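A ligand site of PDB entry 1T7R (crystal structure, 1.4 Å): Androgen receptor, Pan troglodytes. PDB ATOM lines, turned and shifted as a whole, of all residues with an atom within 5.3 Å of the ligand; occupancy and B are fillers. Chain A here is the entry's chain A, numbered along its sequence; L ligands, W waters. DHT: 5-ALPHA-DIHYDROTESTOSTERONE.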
ATOM      1  N   LEU A  51      -4.649   9.718   5.262  1.00  0.00           N
ATOM      2  CA  LEU A  51      -6.020   9.292   4.965  1.00  0.00           C
ATOM      3  C   LEU A  51      -6.370   7.994   5.687  1.00  0.00           C
ATOM      4  O   LEU A  51      -7.510   7.812   6.124  1.00  0.00           O
ATOM      5  CB  LEU A  51      -6.223   9.147   3.445  1.00  0.00           C
ATOM      6  CG  LEU A  51      -6.700  10.432   2.749  1.00  0.00           C
ATOM      7  CD1 LEU A  51      -8.118  10.764   3.222  1.00  0.00           C
ATOM      8  CD2 LEU A  51      -5.759  11.592   3.043  1.00  0.00           C
ATOM      9  N   LEU A  54      -7.329   9.114   9.047  1.00  0.00           N
ATOM     10  CA  LEU A  54      -8.627   9.793   9.068  1.00  0.00           C
ATOM     11  C   LEU A  54      -9.733   8.732   8.989  1.00  0.00           C
ATOM     12  O   LEU A  54     -10.756   8.862   9.654  1.00  0.00           O
ATOM     13  CB  LEU A  54      -8.758  10.792   7.918  1.00  0.00           C
ATOM     14  CG  LEU A  54      -8.054  12.141   8.111  1.00  0.00           C
ATOM     15  CD1 LEU A  54      -8.008  12.886   6.788  1.00  0.00           C
ATOM     16  CD2 LEU A  54      -8.768  12.968   9.183  1.00  0.00           C
ATOM     17  N   ASN A  55      -9.534   7.686   8.184  1.00  0.00           N
ATOM     18  CA  ASN A  55     -10.527   6.628   8.066  1.00  0.00           C
ATOM     19  C   ASN A  55     -10.706   5.876   9.388  1.00  0.00           C
ATOM     20  O   ASN A  55     -11.831   5.566   9.779  1.00  0.00           O
ATOM     21  CB  ASN A  55     -10.145   5.615   6.973  1.00  0.00           C
ATOM     22  CG  ASN A  55     -10.318   6.179   5.580  1.00  0.00           C
ATOM     23  OD1 ASN A  55     -11.092   7.119   5.366  1.00  0.00           O
ATOM     24  ND2 ASN A  55      -9.610   5.594   4.610  1.00  0.00           N
ATOM     25  N   LEU A  57     -10.058   7.101  12.298  1.00  0.00           N
ATOM     26  CA  LEU A  57     -10.699   8.051  13.206  1.00  0.00           C
ATOM     27  C   LEU A  57     -12.195   8.077  12.923  1.00  0.00           C
ATOM     28  O   LEU A  57     -13.002   8.160  13.846  1.00  0.00           O
ATOM     29  CB  LEU A  57     -10.119   9.457  13.031  1.00  0.00           C
ATOM     30  CG  LEU A  57     -10.785  10.537  13.907  1.00  0.00           C
ATOM     31  CD1 LEU A  57     -10.503  10.248  15.385  1.00  0.00           C
ATOM     32  CD2 LEU A  57     -10.232  11.904  13.529  1.00  0.00           C
ATOM     33  N   GLY A  58     -12.556   8.001  11.646  1.00  0.00           N
ATOM     34  CA  GLY A  58     -13.959   7.996  11.271  1.00  0.00           C
ATOM     35  C   GLY A  58     -14.698   6.834  11.908  1.00  0.00           C
ATOM     36  O   GLY A  58     -15.789   6.992  12.454  1.00  0.00           O
ATOM     37  N   GLN A  61     -14.929   7.352  15.760  1.00  0.00           N
ATOM     38  CA  GLN A  61     -15.945   8.341  16.099  1.00  0.00           C
ATOM     39  C   GLN A  61     -17.350   7.810  15.826  1.00  0.00           C
ATOM     40  O   GLN A  61     -18.281   8.170  16.543  1.00  0.00           O
ATOM     41  CB  GLN A  61     -15.721   9.648  15.327  1.00  0.00           C
ATOM     42  CG  GLN A  61     -14.478  10.415  15.781  1.00  0.00           C
ATOM     43  CD  GLN A  61     -14.448  11.842  15.275  1.00  0.00           C
ATOM     44  OE1 GLN A  61     -13.457  12.563  15.466  1.00  0.00           O
ATOM     45  NE2 GLN A  61     -15.530  12.271  14.643  1.00  0.00           N
ATOM     46  N   TRP A  91     -23.649  11.076   9.508  1.00  0.00           N
ATOM     47  CA  TRP A  91     -22.380  11.058  10.232  1.00  0.00           C
ATOM     48  C   TRP A  91     -21.320  12.022   9.725  1.00  0.00           C
ATOM     49  O   TRP A  91     -20.593  12.607  10.529  1.00  0.00           O
ATOM     50  CB  TRP A  91     -21.790   9.628  10.309  1.00  0.00           C
ATOM     51  CG  TRP A  91     -21.480   9.002   8.996  1.00  0.00           C
ATOM     52  CD1 TRP A  91     -22.322   8.269   8.214  1.00  0.00           C
ATOM     53  CD2 TRP A  91     -20.237   9.092   8.284  1.00  0.00           C
ATOM     54  NE1 TRP A  91     -21.687   7.880   7.064  1.00  0.00           N
ATOM     55  CE2 TRP A  91     -20.401   8.371   7.074  1.00  0.00           C
ATOM     56  CE3 TRP A  91     -19.006   9.690   8.539  1.00  0.00           C
ATOM     57  CZ2 TRP A  91     -19.384   8.244   6.119  1.00  0.00           C
ATOM     58  CZ3 TRP A  91     -17.982   9.575   7.595  1.00  0.00           C
ATOM     59  CH2 TRP A  91     -18.177   8.854   6.405  1.00  0.00           C
ATOM     60  N   MET A  92     -21.214  12.212   8.413  1.00  0.00           N
ATOM     61  CA  MET A  92     -20.198  13.112   7.883  1.00  0.00           C
ATOM     62  C   MET A  92     -20.424  14.541   8.377  1.00  0.00           C
ATOM     63  O   MET A  92     -19.511  15.183   8.884  1.00  0.00           O
ATOM     64  CB  MET A  92     -20.198  13.097   6.350  1.00  0.00           C
ATOM     65  CG  MET A  92     -19.080  13.938   5.726  1.00  0.00           C
ATOM     66  SD  MET A  92     -17.417  13.236   5.905  1.00  0.00           S
ATOM     67  CE  MET A  92     -17.434  12.033   4.551  1.00  0.00           C
ATOM     68  N   MET A  95     -19.803  14.828  12.209  1.00  0.00           N
ATOM     69  CA  MET A  95     -18.399  14.794  12.553  1.00  0.00           C
ATOM     70  C   MET A  95     -17.634  16.035  12.119  1.00  0.00           C
ATOM     71  O   MET A  95     -16.719  16.471  12.816  1.00  0.00           O
ATOM     72  CB  MET A  95     -17.742  13.540  11.979  1.00  0.00           C
ATOM     73  CG  MET A  95     -18.233  12.270  12.632  1.00  0.00           C
ATOM     74  SD  MET A  95     -17.450  10.831  11.888  1.00  0.00           S
ATOM     75  CE  MET A  95     -18.374   9.508  12.647  1.00  0.00           C
ATOM     76  N   VAL A  96     -17.997  16.597  10.966  1.00  0.00           N
ATOM     77  CA  VAL A  96     -17.336  17.802  10.480  1.00  0.00           C
ATOM     78  C   VAL A  96     -17.696  18.974  11.401  1.00  0.00           C
ATOM     79  O   VAL A  96     -16.834  19.776  11.776  1.00  0.00           O
ATOM     80  CB  VAL A  96     -17.769  18.110   9.033  1.00  0.00           C
ATOM     81  CG1 VAL A  96     -17.375  19.527   8.637  1.00  0.00           C
ATOM     82  CG2 VAL A  96     -17.121  17.101   8.091  1.00  0.00           C
ATOM     83  N   MET A  99     -15.832  18.630  14.614  1.00  0.00           N
ATOM     84  CA  MET A  99     -14.406  18.890  14.401  1.00  0.00           C
ATOM     85  C   MET A  99     -14.175  20.392  14.310  1.00  0.00           C
ATOM     86  O   MET A  99     -13.188  20.918  14.842  1.00  0.00           O
ATOM     87  CB  MET A  99     -13.933  18.161  13.143  1.00  0.00           C
ATOM     88  CG  MET A  99     -12.425  18.238  12.882  1.00  0.00           C
ATOM     89  SD  MET A  99     -11.937  19.756  12.051  1.00  0.00           S
ATOM     90  CE  MET A  99     -12.586  19.431  10.430  1.00  0.00           C
ATOM     91  N   ARG A 102     -14.173  21.742  17.766  1.00  0.00           N
ATOM     92  CA  ARG A 102     -12.915  21.390  18.452  1.00  0.00           C
ATOM     93  C   ARG A 102     -11.788  22.297  17.992  1.00  0.00           C
ATOM     94  O   ARG A 102     -10.946  22.728  18.799  1.00  0.00           O
ATOM     95  CB  ARG A 102     -12.503  19.951  18.158  1.00  0.00           C
ATOM     96  CG  ARG A 102     -13.278  18.878  18.891  1.00  0.00           C
ATOM     97  CD  ARG A 102     -12.530  17.561  18.844  1.00  0.00           C
ATOM     98  NE  ARG A 102     -12.400  16.990  17.503  1.00  0.00           N
ATOM     99  CZ  ARG A 102     -13.397  16.395  16.838  1.00  0.00           C
ATOM    100  NH1 ARG A 102     -14.605  16.302  17.390  1.00  0.00           N
ATOM    101  NH2 ARG A 102     -13.180  15.872  15.640  1.00  0.00           N
ATOM    102  N   PHE A 114      -8.753  17.374  14.110  1.00  0.00           N
ATOM    103  CA  PHE A 114      -9.498  16.140  13.893  1.00  0.00           C
ATOM    104  C   PHE A 114      -9.469  15.313  15.172  1.00  0.00           C
ATOM    105  O   PHE A 114     -10.476  14.763  15.600  1.00  0.00           O
ATOM    106  CB  PHE A 114      -8.900  15.325  12.741  1.00  0.00           C
ATOM    107  CG  PHE A 114      -9.121  15.947  11.381  1.00  0.00           C
ATOM    108  CD1 PHE A 114     -10.369  15.924  10.775  1.00  0.00           C
ATOM    109  CD2 PHE A 114      -8.065  16.565  10.705  1.00  0.00           C
ATOM    110  CE1 PHE A 114     -10.579  16.501   9.522  1.00  0.00           C
ATOM    111  CE2 PHE A 114      -8.263  17.136   9.453  1.00  0.00           C
ATOM    112  CZ  PHE A 114      -9.521  17.109   8.857  1.00  0.00           C
ATOM    113  N   MET A 130      -7.128  17.136  -0.227  1.00  0.00           N
ATOM    114  CA  MET A 130      -8.470  17.704  -0.101  1.00  0.00           C
ATOM    115  C   MET A 130      -8.336  19.056   0.581  1.00  0.00           C
ATOM    116  O   MET A 130      -9.045  19.383   1.527  1.00  0.00           O
ATOM    117  CB  MET A 130      -9.422  16.748   0.627  1.00  0.00           C
ATOM    118  CG  MET A 130      -8.857  16.123   1.888  1.00  0.00           C
ATOM    119  SD  MET A 130     -10.092  15.093   2.741  1.00  0.00           S
ATOM    120  CE  MET A 130     -10.713  16.252   3.931  1.00  0.00           C
ATOM    121  N   MET A 137     -13.586  23.837   5.820  1.00  0.00           N
ATOM    122  CA  MET A 137     -13.831  23.398   7.188  1.00  0.00           C
ATOM    123  C   MET A 137     -13.183  24.369   8.173  1.00  0.00           C
ATOM    124  O   MET A 137     -13.695  24.575   9.283  1.00  0.00           O
ATOM    125  CB  MET A 137     -13.307  21.973   7.416  1.00  0.00           C
ATOM    126  CG  MET A 137     -14.103  20.919   6.658  1.00  0.00           C
ATOM    127  SD  MET A 137     -13.695  19.223   7.101  1.00  0.00           S
ATOM    128  CE  MET A 137     -12.259  18.934   6.089  1.00  0.00           C
ATOM    129  N   LEU A 223     -16.980  16.040   0.786  1.00  0.00           N
ATOM    130  CA  LEU A 223     -16.241  14.974   1.464  1.00  0.00           C
ATOM    131  C   LEU A 223     -16.825  13.616   1.081  1.00  0.00           C
ATOM    132  O   LEU A 223     -16.077  12.645   0.962  1.00  0.00           O
ATOM    133  CB  LEU A 223     -16.278  15.198   2.967  1.00  0.00           C
ATOM    134  CG  LEU A 223     -15.488  16.444   3.395  1.00  0.00           C
ATOM    135  CD1 LEU A 223     -15.687  16.697   4.880  1.00  0.00           C
ATOM    136  CD2 LEU A 223     -13.999  16.259   3.080  1.00  0.00           C
ATOM    137  N   PHE A 226     -15.336  12.868  -2.218  1.00  0.00           N
ATOM    138  CA  PHE A 226     -13.931  12.544  -2.090  1.00  0.00           C
ATOM    139  C   PHE A 226     -13.703  11.153  -1.501  1.00  0.00           C
ATOM    140  O   PHE A 226     -12.908  10.372  -2.030  1.00  0.00           O
ATOM    141  CB  PHE A 226     -13.233  13.607  -1.232  1.00  0.00           C
ATOM    142  CG  PHE A 226     -11.742  13.421  -1.106  1.00  0.00           C
ATOM    143  CD1 PHE A 226     -11.209  12.663  -0.063  1.00  0.00           C
ATOM    144  CD2 PHE A 226     -10.879  13.998  -2.025  1.00  0.00           C
ATOM    145  CE1 PHE A 226      -9.830  12.509   0.064  1.00  0.00           C
ATOM    146  CE2 PHE A 226      -9.500  13.844  -1.908  1.00  0.00           C
ATOM    147  CZ  PHE A 226      -8.969  13.096  -0.864  1.00  0.00           C
ATOM    148  N   THR A 227     -14.411  10.829  -0.419  1.00  0.00           N
ATOM    149  CA  THR A 227     -14.204   9.515   0.194  1.00  0.00           C
ATOM    150  C   THR A 227     -14.699   8.396  -0.707  1.00  0.00           C
ATOM    151  O   THR A 227     -14.122   7.320  -0.732  1.00  0.00           O
ATOM    152  CB  THR A 227     -14.849   9.430   1.609  1.00  0.00           C
ATOM    153  OG1 THR A 227     -14.319   8.295   2.293  1.00  0.00           O
ATOM    154  CG2 THR A 227     -16.369   9.304   1.538  1.00  0.00           C
ATOM    155  N   LEU A 230     -12.091   7.866  -3.250  1.00  0.00           N
ATOM    156  CA  LEU A 230     -10.922   7.274  -2.616  1.00  0.00           C
ATOM    157  C   LEU A 230     -11.127   5.781  -2.365  1.00  0.00           C
ATOM    158  O   LEU A 230     -10.209   4.987  -2.573  1.00  0.00           O
ATOM    159  CB  LEU A 230     -10.603   7.991  -1.306  1.00  0.00           C
ATOM    160  CG  LEU A 230      -9.344   7.553  -0.544  1.00  0.00           C
ATOM    161  CD1 LEU A 230      -8.122   7.657  -1.446  1.00  0.00           C
ATOM    162  CD2 LEU A 230      -9.182   8.428   0.694  1.00  0.00           C
ATOM    163  N   PHE A 241      -9.189   1.291   4.497  1.00  0.00           N
ATOM    164  CA  PHE A 241     -10.533   1.622   4.960  1.00  0.00           C
ATOM    165  C   PHE A 241     -11.025   0.524   5.893  1.00  0.00           C
ATOM    166  O   PHE A 241     -11.038  -0.645   5.511  1.00  0.00           O
ATOM    167  CB  PHE A 241     -11.542   1.703   3.810  1.00  0.00           C
ATOM    168  CG  PHE A 241     -11.546   3.007   3.077  1.00  0.00           C
ATOM    169  CD1 PHE A 241     -10.643   3.257   2.061  1.00  0.00           C
ATOM    170  CD2 PHE A 241     -12.513   3.971   3.374  1.00  0.00           C
ATOM    171  CE1 PHE A 241     -10.679   4.448   1.342  1.00  0.00           C
ATOM    172  CE2 PHE A 241     -12.561   5.168   2.656  1.00  0.00           C
ATOM    173  CZ  PHE A 241     -11.645   5.412   1.640  1.00  0.00           C
ATOM    174  N   MET A 245     -16.429   1.169   7.492  1.00  0.00           N
ATOM    175  CA  MET A 245     -16.443   2.399   6.725  1.00  0.00           C
ATOM    176  C   MET A 245     -16.630   2.081   5.235  1.00  0.00           C
ATOM    177  O   MET A 245     -17.350   2.780   4.529  1.00  0.00           O
ATOM    178  CB  MET A 245     -15.149   3.183   6.940  1.00  0.00           C
ATOM    179  CG  MET A 245     -14.929   3.574   8.393  1.00  0.00           C
ATOM    180  SD  MET A 245     -16.347   4.456   9.075  1.00  0.00           S
ATOM    181  CE  MET A 245     -16.091   6.019   8.337  1.00  0.00           C
ATOM    182  N   ILE A 249     -19.688   3.601   3.052  1.00  0.00           N
ATOM    183  CA  ILE A 249     -19.349   4.439   1.915  1.00  0.00           C
ATOM    184  C   ILE A 249     -19.738   3.829   0.570  1.00  0.00           C
ATOM    185  O   ILE A 249     -19.944   4.559  -0.404  1.00  0.00           O
ATOM    186  CB  ILE A 249     -17.840   4.793   1.948  1.00  0.00           C
ATOM    187  CG1 ILE A 249     -17.553   5.629   3.195  1.00  0.00           C
ATOM    188  CG2 ILE A 249     -17.438   5.560   0.698  1.00  0.00           C
ATOM    189  CD1 ILE A 249     -16.088   5.788   3.538  1.00  0.00           C
HETATM  190  C1  DHT L   1     -13.190  11.935  10.728  1.00  0.00           C
HETATM  191  C2  DHT L   1     -13.790  12.524  12.008  1.00  0.00           C
HETATM  192  C3  DHT L   1     -13.614  14.073  11.919  1.00  0.00           C
HETATM  193  O3  DHT L   1     -13.138  14.654  12.883  1.00  0.00           O
HETATM  194  C4  DHT L   1     -14.021  14.763  10.652  1.00  0.00           C
HETATM  195  C5  DHT L   1     -13.335  14.124   9.410  1.00  0.00           C
HETATM  196  C6  DHT L   1     -13.763  14.821   8.083  1.00  0.00           C
HETATM  197  C7  DHT L   1     -13.028  14.150   6.908  1.00  0.00           C
HETATM  198  C8  DHT L   1     -13.330  12.618   6.797  1.00  0.00           C
HETATM  199  C9  DHT L   1     -12.935  11.930   8.155  1.00  0.00           C
HETATM  200  C10 DHT L   1     -13.670  12.557   9.387  1.00  0.00           C
HETATM  201  C11 DHT L   1     -13.203  10.388   8.013  1.00  0.00           C
HETATM  202  C12 DHT L   1     -12.542   9.686   6.827  1.00  0.00           C
HETATM  203  C13 DHT L   1     -12.792  10.413   5.482  1.00  0.00           C
HETATM  204  C14 DHT L   1     -12.525  11.953   5.664  1.00  0.00           C
HETATM  205  C15 DHT L   1     -12.747  12.474   4.228  1.00  0.00           C
HETATM  206  C16 DHT L   1     -12.001  11.405   3.374  1.00  0.00           C
HETATM  207  C17 DHT L   1     -11.811  10.203   4.343  1.00  0.00           C
HETATM  208  O17 DHT L   1     -12.018   8.968   3.607  1.00  0.00           O
HETATM  209  C18 DHT L   1     -14.270  10.121   5.032  1.00  0.00           C
HETATM  210  C19 DHT L   1     -15.243  12.327   9.230  1.00  0.00           C
HETATM  211  O   HOH W   1     -15.816  14.871  14.868  1.00  0.00           O
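The guanidinium group (NH2) of Arg 102 lies within hydrogen-bond range of an oxygen (O3) of the ligand, at 3.0 Å. An oxygen (O17) of the ligand is in hydrogen-bond range of the side-chain hydroxyl of Thr 227, at 2.7 Å. O17 of the ligand is in hydrogen-bond range of OD1 of Asn 55 (2.7 Å). The side-chain amide oxygen (OE1) of Gln 61 lies close to an oxygen (O3) of the ligand (3.3 Å).
The side-chain amide nitrogen (ND2) of Asn 55 sits close to the backbone carbonyl oxygen (O) of Leu 51 (3.4 Å). NH2 of Arg 102 sits at hydrogen-bond distance from O of Phe 114 (2.9 Å). NH2 of Arg 102 is in hydrogen-bond range of OE1 of Gln 61. NE2 of Gln 61 sits close to SD of Met 95 (3.7 Å).
Water W1 lies within hydrogen-bond range of the side-chain amide nitrogen of Gln 61 (2.6 Å), the backbone carbonyl oxygen of Met 95 (2.8 Å), the guanidinium group of Arg 102 (2.9 Å) and an oxygen (O3) of the ligand (3.3 Å).
CD1 of Leu 51 touches C17 of the ligand, at 3.9 Å. Leu 54 touches the ligand. Leu 57 touches the ligand (CD2 to C2, 3.9 Å). Met 92 touches the ligand. Met 95 touches the ligand (SD to C19, 3.8 Å). CB of Met 99 touches O3 of the ligand (3.6 Å). CE1 of Phe 114 touches C5 of the ligand (3.6 Å). Phe 226 touches the ligand (CD1 to C16, 3.7 Å). Phe 241 touches the ligand (CE2 to O17, 3.95 Å). Hydrophobic or aromatic side chains within 4 Å of the ligand: Leu 51, Leu 57, Met 92, Met 95, Met 99, Phe 114, Phe 226 and Phe 241. Of the 22 residues printed, 13 come within 4 Å of the ligand.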
